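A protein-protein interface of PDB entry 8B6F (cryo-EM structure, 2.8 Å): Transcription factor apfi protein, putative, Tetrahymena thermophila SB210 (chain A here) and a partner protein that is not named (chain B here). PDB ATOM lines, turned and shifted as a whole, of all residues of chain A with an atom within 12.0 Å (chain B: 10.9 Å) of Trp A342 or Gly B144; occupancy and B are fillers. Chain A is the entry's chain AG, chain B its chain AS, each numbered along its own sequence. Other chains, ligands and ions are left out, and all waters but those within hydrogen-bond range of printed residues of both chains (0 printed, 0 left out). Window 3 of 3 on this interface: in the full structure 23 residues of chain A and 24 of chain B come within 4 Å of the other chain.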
ATOM      1  N   PHE A 333      -9.914 -11.255 -25.837  1.00  0.00           N
ATOM      2  CA  PHE A 333     -10.380 -12.391 -26.619  1.00  0.00           C
ATOM      3  C   PHE A 333      -9.475 -12.616 -27.822  1.00  0.00           C
ATOM      4  O   PHE A 333      -9.142 -11.677 -28.550  1.00  0.00           O
ATOM      5  CB  PHE A 333     -11.818 -12.158 -27.077  1.00  0.00           C
ATOM      6  CG  PHE A 333     -12.296 -13.147 -28.101  1.00  0.00           C
ATOM      7  CD1 PHE A 333     -12.849 -14.355 -27.709  1.00  0.00           C
ATOM      8  CD2 PHE A 333     -12.203 -12.865 -29.454  1.00  0.00           C
ATOM      9  CE1 PHE A 333     -13.294 -15.266 -28.649  1.00  0.00           C
ATOM     10  CE2 PHE A 333     -12.645 -13.771 -30.400  1.00  0.00           C
ATOM     11  CZ  PHE A 333     -13.191 -14.974 -29.996  1.00  0.00           C
ATOM     12  N   LYS A 334      -9.083 -13.869 -28.030  1.00  0.00           N
ATOM     13  CA  LYS A 334      -8.255 -14.259 -29.159  1.00  0.00           C
ATOM     14  C   LYS A 334      -8.848 -15.502 -29.801  1.00  0.00           C
ATOM     15  O   LYS A 334      -9.354 -16.388 -29.106  1.00  0.00           O
ATOM     16  CB  LYS A 334      -6.809 -14.528 -28.722  1.00  0.00           C
ATOM     17  CG  LYS A 334      -5.884 -14.933 -29.858  1.00  0.00           C
ATOM     18  CD  LYS A 334      -4.472 -15.192 -29.358  1.00  0.00           C
ATOM     19  CE  LYS A 334      -3.558 -15.627 -30.493  1.00  0.00           C
ATOM     20  NZ  LYS A 334      -2.176 -15.922 -30.018  1.00  0.00           N
ATOM     21  N   GLU A 335      -8.785 -15.561 -31.125  1.00  0.00           N
ATOM     22  CA  GLU A 335      -9.297 -16.725 -31.830  1.00  0.00           C
ATOM     23  C   GLU A 335      -8.491 -17.959 -31.430  1.00  0.00           C
ATOM     24  O   GLU A 335      -7.259 -17.896 -31.350  1.00  0.00           O
ATOM     25  CB  GLU A 335      -9.226 -16.511 -33.341  1.00  0.00           C
ATOM     26  CG  GLU A 335     -10.138 -15.402 -33.841  1.00  0.00           C
ATOM     27  CD  GLU A 335      -9.904 -15.066 -35.300  1.00  0.00           C
ATOM     28  OE1 GLU A 335      -9.013 -15.687 -35.918  1.00  0.00           O
ATOM     29  OE2 GLU A 335     -10.607 -14.179 -35.827  1.00  0.00           O
ATOM     30  N   PRO A 336      -9.144 -19.090 -31.171  1.00  0.00           N
ATOM     31  CA  PRO A 336      -8.404 -20.261 -30.687  1.00  0.00           C
ATOM     32  C   PRO A 336      -7.363 -20.724 -31.693  1.00  0.00           C
ATOM     33  O   PRO A 336      -7.583 -20.693 -32.905  1.00  0.00           O
ATOM     34  CB  PRO A 336      -9.500 -21.313 -30.481  1.00  0.00           C
ATOM     35  CG  PRO A 336     -10.606 -20.889 -31.373  1.00  0.00           C
ATOM     36  CD  PRO A 336     -10.567 -19.394 -31.392  1.00  0.00           C
ATOM     37  N   THR A 337      -6.214 -21.154 -31.171  1.00  0.00           N
ATOM     38  CA  THR A 337      -5.184 -21.725 -32.032  1.00  0.00           C
ATOM     39  C   THR A 337      -5.564 -23.132 -32.472  1.00  0.00           C
ATOM     40  O   THR A 337      -5.318 -23.518 -33.621  1.00  0.00           O
ATOM     41  CB  THR A 337      -3.836 -21.733 -31.311  1.00  0.00           C
ATOM     42  OG1 THR A 337      -3.922 -22.550 -30.135  1.00  0.00           O
ATOM     43  CG2 THR A 337      -3.430 -20.320 -30.917  1.00  0.00           C
ATOM     44  N   ASN A 338      -6.162 -23.910 -31.574  1.00  0.00           N
ATOM     45  CA  ASN A 338      -6.655 -25.249 -31.894  1.00  0.00           C
ATOM     46  C   ASN A 338      -8.126 -25.123 -32.264  1.00  0.00           C
ATOM     47  O   ASN A 338      -8.995 -25.057 -31.393  1.00  0.00           O
ATOM     48  CB  ASN A 338      -6.451 -26.193 -30.716  1.00  0.00           C
ATOM     49  CG  ASN A 338      -7.031 -27.570 -30.967  1.00  0.00           C
ATOM     50  OD1 ASN A 338      -7.267 -27.958 -32.110  1.00  0.00           O
ATOM     51  ND2 ASN A 338      -7.264 -28.317 -29.894  1.00  0.00           N
ATOM     52  N   LYS A 339      -8.407 -25.098 -33.564  1.00  0.00           N
ATOM     53  CA  LYS A 339      -9.754 -24.888 -34.071  1.00  0.00           C
ATOM     54  C   LYS A 339     -10.502 -26.192 -34.308  1.00  0.00           C
ATOM     55  O   LYS A 339     -11.607 -26.166 -34.856  1.00  0.00           O
ATOM     56  CB  LYS A 339      -9.703 -24.076 -35.368  1.00  0.00           C
ATOM     57  CG  LYS A 339      -9.024 -22.724 -35.215  1.00  0.00           C
ATOM     58  CD  LYS A 339      -8.923 -21.993 -36.545  1.00  0.00           C
ATOM     59  CE  LYS A 339      -8.203 -20.662 -36.386  1.00  0.00           C
ATOM     60  NZ  LYS A 339      -8.085 -19.934 -37.680  1.00  0.00           N
ATOM     61  N   LYS A 340      -9.929 -27.325 -33.911  1.00  0.00           N
ATOM     62  CA  LYS A 340     -10.605 -28.603 -34.097  1.00  0.00           C
ATOM     63  C   LYS A 340     -12.011 -28.627 -33.515  1.00  0.00           C
ATOM     64  O   LYS A 340     -12.918 -29.132 -34.195  1.00  0.00           O
ATOM     65  CB  LYS A 340      -9.763 -29.732 -33.487  1.00  0.00           C
ATOM     66  CG  LYS A 340      -8.475 -30.019 -34.235  1.00  0.00           C
ATOM     67  CD  LYS A 340      -7.750 -31.212 -33.634  1.00  0.00           C
ATOM     68  CE  LYS A 340      -6.516 -31.571 -34.442  1.00  0.00           C
ATOM     69  NZ  LYS A 340      -5.819 -32.765 -33.887  1.00  0.00           N
ATOM     70  N   PRO A 341     -12.267 -28.120 -32.307  1.00  0.00           N
ATOM     71  CA  PRO A 341     -13.636 -28.200 -31.774  1.00  0.00           C
ATOM     72  C   PRO A 341     -14.674 -27.565 -32.679  1.00  0.00           C
ATOM     73  O   PRO A 341     -15.797 -28.077 -32.779  1.00  0.00           O
ATOM     74  CB  PRO A 341     -13.527 -27.465 -30.429  1.00  0.00           C
ATOM     75  CG  PRO A 341     -12.097 -27.572 -30.053  1.00  0.00           C
ATOM     76  CD  PRO A 341     -11.334 -27.520 -31.338  1.00  0.00           C
ATOM     77  N   TRP A 342     -14.335 -26.460 -33.340  1.00  0.00           N
ATOM     78  CA  TRP A 342     -15.273 -25.748 -34.196  1.00  0.00           C
ATOM     79  C   TRP A 342     -15.093 -26.062 -35.675  1.00  0.00           C
ATOM     80  O   TRP A 342     -15.822 -25.504 -36.499  1.00  0.00           O
ATOM     81  CB  TRP A 342     -15.136 -24.237 -33.974  1.00  0.00           C
ATOM     82  CG  TRP A 342     -15.286 -23.836 -32.541  1.00  0.00           C
ATOM     83  CD1 TRP A 342     -16.438 -23.476 -31.908  1.00  0.00           C
ATOM     84  CD2 TRP A 342     -14.248 -23.761 -31.558  1.00  0.00           C
ATOM     85  NE1 TRP A 342     -16.181 -23.179 -30.592  1.00  0.00           N
ATOM     86  CE2 TRP A 342     -14.843 -23.346 -30.353  1.00  0.00           C
ATOM     87  CE3 TRP A 342     -12.870 -24.003 -31.582  1.00  0.00           C
ATOM     88  CZ2 TRP A 342     -14.112 -23.168 -29.182  1.00  0.00           C
ATOM     89  CZ3 TRP A 342     -12.145 -23.826 -30.420  1.00  0.00           C
ATOM     90  CH2 TRP A 342     -12.767 -23.412 -29.235  1.00  0.00           C
ATOM     91  N   THR A 343     -14.145 -26.934 -36.035  1.00  0.00           N
ATOM     92  CA  THR A 343     -13.889 -27.252 -37.436  1.00  0.00           C
ATOM     93  C   THR A 343     -13.786 -28.754 -37.684  1.00  0.00           C
ATOM     94  O   THR A 343     -13.285 -29.166 -38.736  1.00  0.00           O
ATOM     95  CB  THR A 343     -12.614 -26.560 -37.922  1.00  0.00           C
ATOM     96  OG1 THR A 343     -11.496 -27.003 -37.142  1.00  0.00           O
ATOM     97  CG2 THR A 343     -12.743 -25.050 -37.802  1.00  0.00           C
ATOM     98  N   ARG A 344     -14.244 -29.580 -36.750  1.00  0.00           N
ATOM     99  CA  ARG A 344     -14.258 -31.027 -36.916  1.00  0.00           C
ATOM    100  C   ARG A 344     -15.660 -31.479 -37.298  1.00  0.00           C
ATOM    101  O   ARG A 344     -16.649 -31.002 -36.738  1.00  0.00           O
ATOM    102  CB  ARG A 344     -13.803 -31.742 -35.642  1.00  0.00           C
ATOM    103  CG  ARG A 344     -14.723 -31.521 -34.468  1.00  0.00           C
ATOM    104  CD  ARG A 344     -14.279 -32.255 -33.215  1.00  0.00           C
ATOM    105  NE  ARG A 344     -14.430 -33.698 -33.351  1.00  0.00           N
ATOM    106  CZ  ARG A 344     -14.320 -34.561 -32.351  1.00  0.00           C
ATOM    107  NH1 ARG A 344     -14.058 -34.160 -31.117  1.00  0.00           N
ATOM    108  NH2 ARG A 344     -14.482 -35.858 -32.593  1.00  0.00           N
ATOM    109  N   LYS A 345     -15.741 -32.396 -38.258  1.00  0.00           N
ATOM    110  CA  LYS A 345     -17.017 -32.963 -38.674  1.00  0.00           C
ATOM    111  C   LYS A 345     -17.326 -34.284 -37.987  1.00  0.00           C
ATOM    112  O   LYS A 345     -18.464 -34.502 -37.563  1.00  0.00           O
ATOM    113  CB  LYS A 345     -17.040 -33.165 -40.193  1.00  0.00           C
ATOM    114  CG  LYS A 345     -18.404 -33.565 -40.736  1.00  0.00           C
ATOM    115  CD  LYS A 345     -18.396 -33.654 -42.251  1.00  0.00           C
ATOM    116  CE  LYS A 345     -19.751 -34.093 -42.782  1.00  0.00           C
ATOM    117  NZ  LYS A 345     -19.753 -34.226 -44.266  1.00  0.00           N
ATOM    118  N   TYR A 346     -16.343 -35.170 -37.865  1.00  0.00           N
ATOM    119  CA  TYR A 346     -16.544 -36.454 -37.203  1.00  0.00           C
ATOM    120  C   TYR A 346     -15.621 -36.590 -36.001  1.00  0.00           C
ATOM    121  O   TYR A 346     -15.941 -37.276 -35.032  1.00  0.00           O
ATOM    122  CB  TYR A 346     -16.300 -37.603 -38.180  1.00  0.00           C
ATOM    123  CG  TYR A 346     -17.192 -37.569 -39.397  1.00  0.00           C
ATOM    124  CD1 TYR A 346     -18.484 -38.072 -39.348  1.00  0.00           C
ATOM    125  CD2 TYR A 346     -16.738 -37.037 -40.596  1.00  0.00           C
ATOM    126  CE1 TYR A 346     -19.304 -38.045 -40.459  1.00  0.00           C
ATOM    127  CE2 TYR A 346     -17.548 -37.004 -41.712  1.00  0.00           C
ATOM    128  CZ  TYR A 346     -18.830 -37.508 -41.638  1.00  0.00           C
ATOM    129  OH  TYR A 346     -19.640 -37.480 -42.749  1.00  0.00           O
ATOM    130  OXT TYR A 346     -14.533 -36.017 -35.967  1.00  0.00           O
ATOM    131  N   GLY B  77     -13.885 -33.010 -19.724  1.00  0.00           N
ATOM    132  CA  GLY B  77     -12.923 -33.227 -20.790  1.00  0.00           C
ATOM    133  C   GLY B  77     -13.267 -32.473 -22.058  1.00  0.00           C
ATOM    134  O   GLY B  77     -12.373 -32.021 -22.778  1.00  0.00           O
ATOM    135  N   THR B  78     -14.560 -32.334 -22.355  1.00  0.00           N
ATOM    136  CA  THR B  78     -14.972 -31.624 -23.562  1.00  0.00           C
ATOM    137  C   THR B  78     -14.585 -30.151 -23.497  1.00  0.00           C
ATOM    138  O   THR B  78     -14.184 -29.562 -24.507  1.00  0.00           O
ATOM    139  CB  THR B  78     -16.480 -31.767 -23.762  1.00  0.00           C
ATOM    140  OG1 THR B  78     -16.840 -33.154 -23.715  1.00  0.00           O
ATOM    141  CG2 THR B  78     -16.904 -31.188 -25.102  1.00  0.00           C
ATOM    142  N   LYS B  79     -14.703 -29.538 -22.318  1.00  0.00           N
ATOM    143  CA  LYS B  79     -14.417 -28.112 -22.195  1.00  0.00           C
ATOM    144  C   LYS B  79     -12.974 -27.803 -22.566  1.00  0.00           C
ATOM    145  O   LYS B  79     -12.695 -26.783 -23.208  1.00  0.00           O
ATOM    146  CB  LYS B  79     -14.716 -27.640 -20.773  1.00  0.00           C
ATOM    147  CG  LYS B  79     -16.197 -27.617 -20.430  1.00  0.00           C
ATOM    148  CD  LYS B  79     -16.425 -27.257 -18.972  1.00  0.00           C
ATOM    149  CE  LYS B  79     -17.908 -27.172 -18.648  1.00  0.00           C
ATOM    150  NZ  LYS B  79     -18.613 -28.463 -18.891  1.00  0.00           N
ATOM    151  N   PHE B  80     -12.042 -28.661 -22.166  1.00  0.00           N
ATOM    152  CA  PHE B  80     -10.636 -28.455 -22.481  1.00  0.00           C
ATOM    153  C   PHE B  80      -9.921 -29.797 -22.459  1.00  0.00           C
ATOM    154  O   PHE B  80     -10.300 -30.705 -21.719  1.00  0.00           O
ATOM    155  CB  PHE B  80      -9.981 -27.482 -21.493  1.00  0.00           C
ATOM    156  CG  PHE B  80     -10.635 -27.462 -20.142  1.00  0.00           C
ATOM    157  CD1 PHE B  80     -10.575 -28.567 -19.313  1.00  0.00           C
ATOM    158  CD2 PHE B  80     -11.300 -26.333 -19.698  1.00  0.00           C
ATOM    159  CE1 PHE B  80     -11.175 -28.550 -18.071  1.00  0.00           C
ATOM    160  CE2 PHE B  80     -11.901 -26.309 -18.456  1.00  0.00           C
ATOM    161  CZ  PHE B  80     -11.839 -27.420 -17.642  1.00  0.00           C
ATOM    162  N   THR B  81      -8.889 -29.909 -23.289  1.00  0.00           N
ATOM    163  CA  THR B  81      -8.061 -31.103 -23.298  1.00  0.00           C
ATOM    164  C   THR B  81      -7.168 -31.129 -22.061  1.00  0.00           C
ATOM    165  O   THR B  81      -6.974 -30.119 -21.381  1.00  0.00           O
ATOM    166  CB  THR B  81      -7.209 -31.146 -24.570  1.00  0.00           C
ATOM    167  OG1 THR B  81      -8.024 -30.830 -25.704  1.00  0.00           O
ATOM    168  CG2 THR B  81      -6.596 -32.524 -24.781  1.00  0.00           C
ATOM    169  N   GLN B  84      -4.459 -28.736 -22.469  1.00  0.00           N
ATOM    170  CA  GLN B  84      -4.972 -27.378 -22.332  1.00  0.00           C
ATOM    171  C   GLN B  84      -5.146 -27.008 -20.865  1.00  0.00           C
ATOM    172  O   GLN B  84      -4.795 -25.899 -20.451  1.00  0.00           O
ATOM    173  CB  GLN B  84      -6.292 -27.234 -23.087  1.00  0.00           C
ATOM    174  CG  GLN B  84      -6.138 -27.320 -24.596  1.00  0.00           C
ATOM    175  CD  GLN B  84      -7.465 -27.265 -25.321  1.00  0.00           C
ATOM    176  OE1 GLN B  84      -8.508 -27.583 -24.754  1.00  0.00           O
ATOM    177  NE2 GLN B  84      -7.433 -26.850 -26.581  1.00  0.00           N
ATOM    178  N   PRO B 135      -9.282 -21.407 -19.970  1.00  0.00           N
ATOM    179  CA  PRO B 135      -8.312 -20.600 -20.718  1.00  0.00           C
ATOM    180  C   PRO B 135      -8.411 -19.126 -20.354  1.00  0.00           C
ATOM    181  O   PRO B 135      -9.484 -18.612 -20.035  1.00  0.00           O
ATOM    182  CB  PRO B 135      -8.698 -20.838 -22.183  1.00  0.00           C
ATOM    183  CG  PRO B 135      -9.521 -22.071 -22.178  1.00  0.00           C
ATOM    184  CD  PRO B 135     -10.233 -22.083 -20.869  1.00  0.00           C
ATOM    185  N   ASN B 137      -7.525 -16.510 -22.456  1.00  0.00           N
ATOM    186  CA  ASN B 137      -7.979 -15.701 -23.581  1.00  0.00           C
ATOM    187  C   ASN B 137      -8.528 -16.538 -24.729  1.00  0.00           C
ATOM    188  O   ASN B 137      -8.788 -15.985 -25.804  1.00  0.00           O
ATOM    189  CB  ASN B 137      -6.838 -14.816 -24.093  1.00  0.00           C
ATOM    190  CG  ASN B 137      -5.612 -15.613 -24.478  1.00  0.00           C
ATOM    191  OD1 ASN B 137      -5.331 -16.660 -23.898  1.00  0.00           O
ATOM    192  ND2 ASN B 137      -4.869 -15.116 -25.460  1.00  0.00           N
ATOM    193  N   THR B 138      -8.721 -17.841 -24.540  1.00  0.00           N
ATOM    194  CA  THR B 138      -9.218 -18.718 -25.583  1.00  0.00           C
ATOM    195  C   THR B 138     -10.635 -19.184 -25.257  1.00  0.00           C
ATOM    196  O   THR B 138     -10.975 -19.363 -24.083  1.00  0.00           O
ATOM    197  CB  THR B 138      -8.306 -19.942 -25.742  1.00  0.00           C
ATOM    198  OG1 THR B 138      -6.955 -19.512 -25.960  1.00  0.00           O
ATOM    199  CG2 THR B 138      -8.751 -20.813 -26.908  1.00  0.00           C
ATOM    200  N   PRO B 139     -11.489 -19.379 -26.259  1.00  0.00           N
ATOM    201  CA  PRO B 139     -12.842 -19.865 -25.975  1.00  0.00           C
ATOM    202  C   PRO B 139     -12.838 -21.272 -25.403  1.00  0.00           C
ATOM    203  O   PRO B 139     -11.943 -22.078 -25.666  1.00  0.00           O
ATOM    204  CB  PRO B 139     -13.527 -19.834 -27.346  1.00  0.00           C
ATOM    205  CG  PRO B 139     -12.735 -18.887 -28.154  1.00  0.00           C
ATOM    206  CD  PRO B 139     -11.328 -19.027 -27.680  1.00  0.00           C
ATOM    207  N   LEU B 140     -13.861 -21.558 -24.603  1.00  0.00           N
ATOM    208  CA  LEU B 140     -14.065 -22.910 -24.106  1.00  0.00           C
ATOM    209  C   LEU B 140     -14.423 -23.834 -25.264  1.00  0.00           C
ATOM    210  O   LEU B 140     -15.175 -23.460 -26.167  1.00  0.00           O
ATOM    211  CB  LEU B 140     -15.167 -22.922 -23.047  1.00  0.00           C
ATOM    212  CG  LEU B 140     -14.984 -23.860 -21.850  1.00  0.00           C
ATOM    213  CD1 LEU B 140     -13.728 -23.514 -21.059  1.00  0.00           C
ATOM    214  CD2 LEU B 140     -16.203 -23.811 -20.946  1.00  0.00           C
ATOM    215  N   SER B 141     -13.879 -25.052 -25.236  1.00  0.00           N
ATOM    216  CA  SER B 141     -13.975 -25.945 -26.385  1.00  0.00           C
ATOM    217  C   SER B 141     -15.355 -26.567 -26.560  1.00  0.00           C
ATOM    218  O   SER B 141     -15.608 -27.169 -27.609  1.00  0.00           O
ATOM    219  CB  SER B 141     -12.936 -27.062 -26.266  1.00  0.00           C
ATOM    220  OG  SER B 141     -11.622 -26.536 -26.198  1.00  0.00           O
ATOM    221  N   ASP B 142     -16.244 -26.446 -25.580  1.00  0.00           N
ATOM    222  CA  ASP B 142     -17.569 -27.049 -25.651  1.00  0.00           C
ATOM    223  C   ASP B 142     -18.652 -26.050 -26.033  1.00  0.00           C
ATOM    224  O   ASP B 142     -19.838 -26.385 -25.967  1.00  0.00           O
ATOM    225  CB  ASP B 142     -17.920 -27.706 -24.316  1.00  0.00           C
ATOM    226  CG  ASP B 142     -18.021 -26.705 -23.189  1.00  0.00           C
ATOM    227  OD1 ASP B 142     -17.254 -25.720 -23.203  1.00  0.00           O
ATOM    228  OD2 ASP B 142     -18.863 -26.901 -22.288  1.00  0.00           O
ATOM    229  N   ARG B 143     -18.277 -24.837 -26.427  1.00  0.00           N
ATOM    230  CA  ARG B 143     -19.230 -23.783 -26.731  1.00  0.00           C
ATOM    231  C   ARG B 143     -18.836 -23.089 -28.024  1.00  0.00           C
ATOM    232  O   ARG B 143     -17.669 -23.088 -28.424  1.00  0.00           O
ATOM    233  CB  ARG B 143     -19.301 -22.745 -25.602  1.00  0.00           C
ATOM    234  CG  ARG B 143     -19.775 -23.290 -24.270  1.00  0.00           C
ATOM    235  CD  ARG B 143     -19.471 -22.307 -23.152  1.00  0.00           C
ATOM    236  NE  ARG B 143     -20.131 -22.670 -21.905  1.00  0.00           N
ATOM    237  CZ  ARG B 143     -21.349 -22.280 -21.557  1.00  0.00           C
ATOM    238  NH1 ARG B 143     -22.084 -21.513 -22.347  1.00  0.00           N
ATOM    239  NH2 ARG B 143     -21.845 -22.668 -20.385  1.00  0.00           N
ATOM    240  N   GLY B 144     -19.830 -22.500 -28.678  1.00  0.00           N
ATOM    241  CA  GLY B 144     -19.574 -21.653 -29.822  1.00  0.00           C
ATOM    242  C   GLY B 144     -19.315 -20.227 -29.389  1.00  0.00           C
ATOM    243  O   GLY B 144     -20.135 -19.630 -28.687  1.00  0.00           O
ATOM    244  N   TYR B 145     -18.180 -19.671 -29.792  1.00  0.00           N
ATOM    245  CA  TYR B 145     -17.787 -18.344 -29.350  1.00  0.00           C
ATOM    246  C   TYR B 145     -18.304 -17.275 -30.304  1.00  0.00           C
ATOM    247  O   TYR B 145     -18.652 -17.542 -31.455  1.00  0.00           O
ATOM    248  CB  TYR B 145     -16.267 -18.244 -29.224  1.00  0.00           C
ATOM    249  CG  TYR B 145     -15.515 -18.543 -30.498  1.00  0.00           C
ATOM    250  CD1 TYR B 145     -15.251 -17.546 -31.424  1.00  0.00           C
ATOM    251  CD2 TYR B 145     -15.055 -19.823 -30.765  1.00  0.00           C
ATOM    252  CE1 TYR B 145     -14.559 -17.817 -32.585  1.00  0.00           C
ATOM    253  CE2 TYR B 145     -14.362 -20.104 -31.921  1.00  0.00           C
ATOM    254  CZ  TYR B 145     -14.117 -19.098 -32.827  1.00  0.00           C
ATOM    255  OH  TYR B 145     -13.426 -19.377 -33.982  1.00  0.00           O
ATOM    256  N   SER B 146     -18.347 -16.047 -29.800  1.00  0.00           N
ATOM    257  CA  SER B 146     -18.793 -14.886 -30.558  1.00  0.00           C
ATOM    258  C   SER B 146     -17.595 -13.986 -30.816  1.00  0.00           C
ATOM    259  O   SER B 146     -16.947 -13.524 -29.871  1.00  0.00           O
ATOM    260  CB  SER B 146     -19.881 -14.130 -29.797  1.00  0.00           C
ATOM    261  OG  SER B 146     -20.160 -12.882 -30.408  1.00  0.00           O
ATOM    262  N   TYR B 147     -17.307 -13.736 -32.093  1.00  0.00           N
ATOM    263  CA  TYR B 147     -16.237 -12.832 -32.498  1.00  0.00           C
ATOM    264  C   TYR B 147     -16.785 -11.502 -33.005  1.00  0.00           C
ATOM    265  O   TYR B 147     -16.105 -10.800 -33.758  1.00  0.00           O
ATOM    266  CB  TYR B 147     -15.352 -13.488 -33.559  1.00  0.00           C
ATOM    267  CG  TYR B 147     -16.109 -14.063 -34.733  1.00  0.00           C
ATOM    268  CD1 TYR B 147     -16.570 -15.372 -34.714  1.00  0.00           C
ATOM    269  CD2 TYR B 147     -16.355 -13.300 -35.862  1.00  0.00           C
ATOM    270  CE1 TYR B 147     -17.260 -15.900 -35.785  1.00  0.00           C
ATOM    271  CE2 TYR B 147     -17.043 -13.818 -36.940  1.00  0.00           C
ATOM    272  CZ  TYR B 147     -17.493 -15.119 -36.895  1.00  0.00           C
ATOM    273  OH  TYR B 147     -18.179 -15.637 -37.966  1.00  0.00           O
ATOM    274  N   LEU B 148     -18.005 -11.144 -32.601  1.00  0.00           N
ATOM    275  CA  LEU B 148     -18.579  -9.868 -33.012  1.00  0.00           C
ATOM    276  C   LEU B 148     -17.730  -8.705 -32.526  1.00  0.00           C
ATOM    277  O   LEU B 148     -17.481  -7.752 -33.274  1.00  0.00           O
ATOM    278  CB  LEU B 148     -20.010  -9.748 -32.482  1.00  0.00           C
ATOM    279  CG  LEU B 148     -20.735  -8.404 -32.636  1.00  0.00           C
ATOM    280  CD1 LEU B 148     -22.231  -8.633 -32.689  1.00  0.00           C
ATOM    281  CD2 LEU B 148     -20.421  -7.435 -31.502  1.00  0.00           C
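Gly B144 touches one residue of chain A.
Printed residues of chain B within 4 Å of Pro A336: Thr B138, Pro B139 and Tyr B145.
No residue of chain B comes within 4 Å of Thr A343.
Of the printed residues of chain A, Pro B139 touches Phe A333 (3.7 Å), Lys A334 (3.6 Å), Pro A336 (3.8 Å) and Trp A342 (3.9 Å).
Ser B141 touches just these residues of chain A: Pro A341 (3.5 Å) and Trp A342 (3.9 Å).
No residue of chain A comes within 4 Å of Asp B142.
Printed residues of chain A within 4 Å of Tyr B145: Phe A333 (3.6 Å), Pro A336 (3.8 Å) and Trp A342 (3.5 Å).
No residue of chain A comes within 4 Å of Ser B146.
Of the printed residues of chain B, Lys A334 touches Asn B137 (3.1 Å) and Pro B139 (3.6 Å).
Of the printed residues of chain A, Asn B137 touches Phe A333 and Lys A334.
Printed residues of chain A within 4 Å of Gln B84: Asn A338 (3.6 Å).
Of the printed residues of chain A, Arg B143 touches Trp A342 (2.6 Å).
Pro B135 touches none of the printed residues of chain A.
Lys B79 touches none of the printed residues of chain A.
The nearest printed residue of chain B that does not touch Phe A333 is Ser B146 (4.03 Å).
O of Lys B79 lies within hydrogen-bond range of N of Ser B141, at 2.9 Å.
N of Thr B81 is in hydrogen-bond range of OE1 of Gln B84 (2.8 Å).
The side-chain amide oxygen (OD1) of Asn A338 sits close to the backbone NH (N) of Lys A340, 3.3 Å away.
Among the printed residues, merely in contact across the chains: Trp A342 with Leu B140, Pro A341 with Ser B141, Trp A342 with Tyr B145, Lys A334 with Pro B139, Phe A333 with Tyr B145, Asn A338 with Gln B84, Pro A336 with Thr B138, Phe A333 with Pro B139, Trp A342 with Gly B144, Pro A336 with Pro B139, Pro A336 with Tyr B145, Trp A342 with Pro B139, Trp A342 with Ser B141 and Phe A333 with Asn B137.
Hydrophobic or aromatic side chains of chain A that line the printed part of chain B: Phe A333, Pro A336, Pro A341 and Trp A342.
Among the printed residues, no Asp or Glu carboxylate lies within 4 Å of a Lys or Arg side-chain nitrogen of the other chain.
O of Asn B137 is in hydrogen-bond range of N of Lys A334, at 3.1 Å.
NE1 of Trp A342 lies within hydrogen-bond range of O of Arg B143 (2.6 Å).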
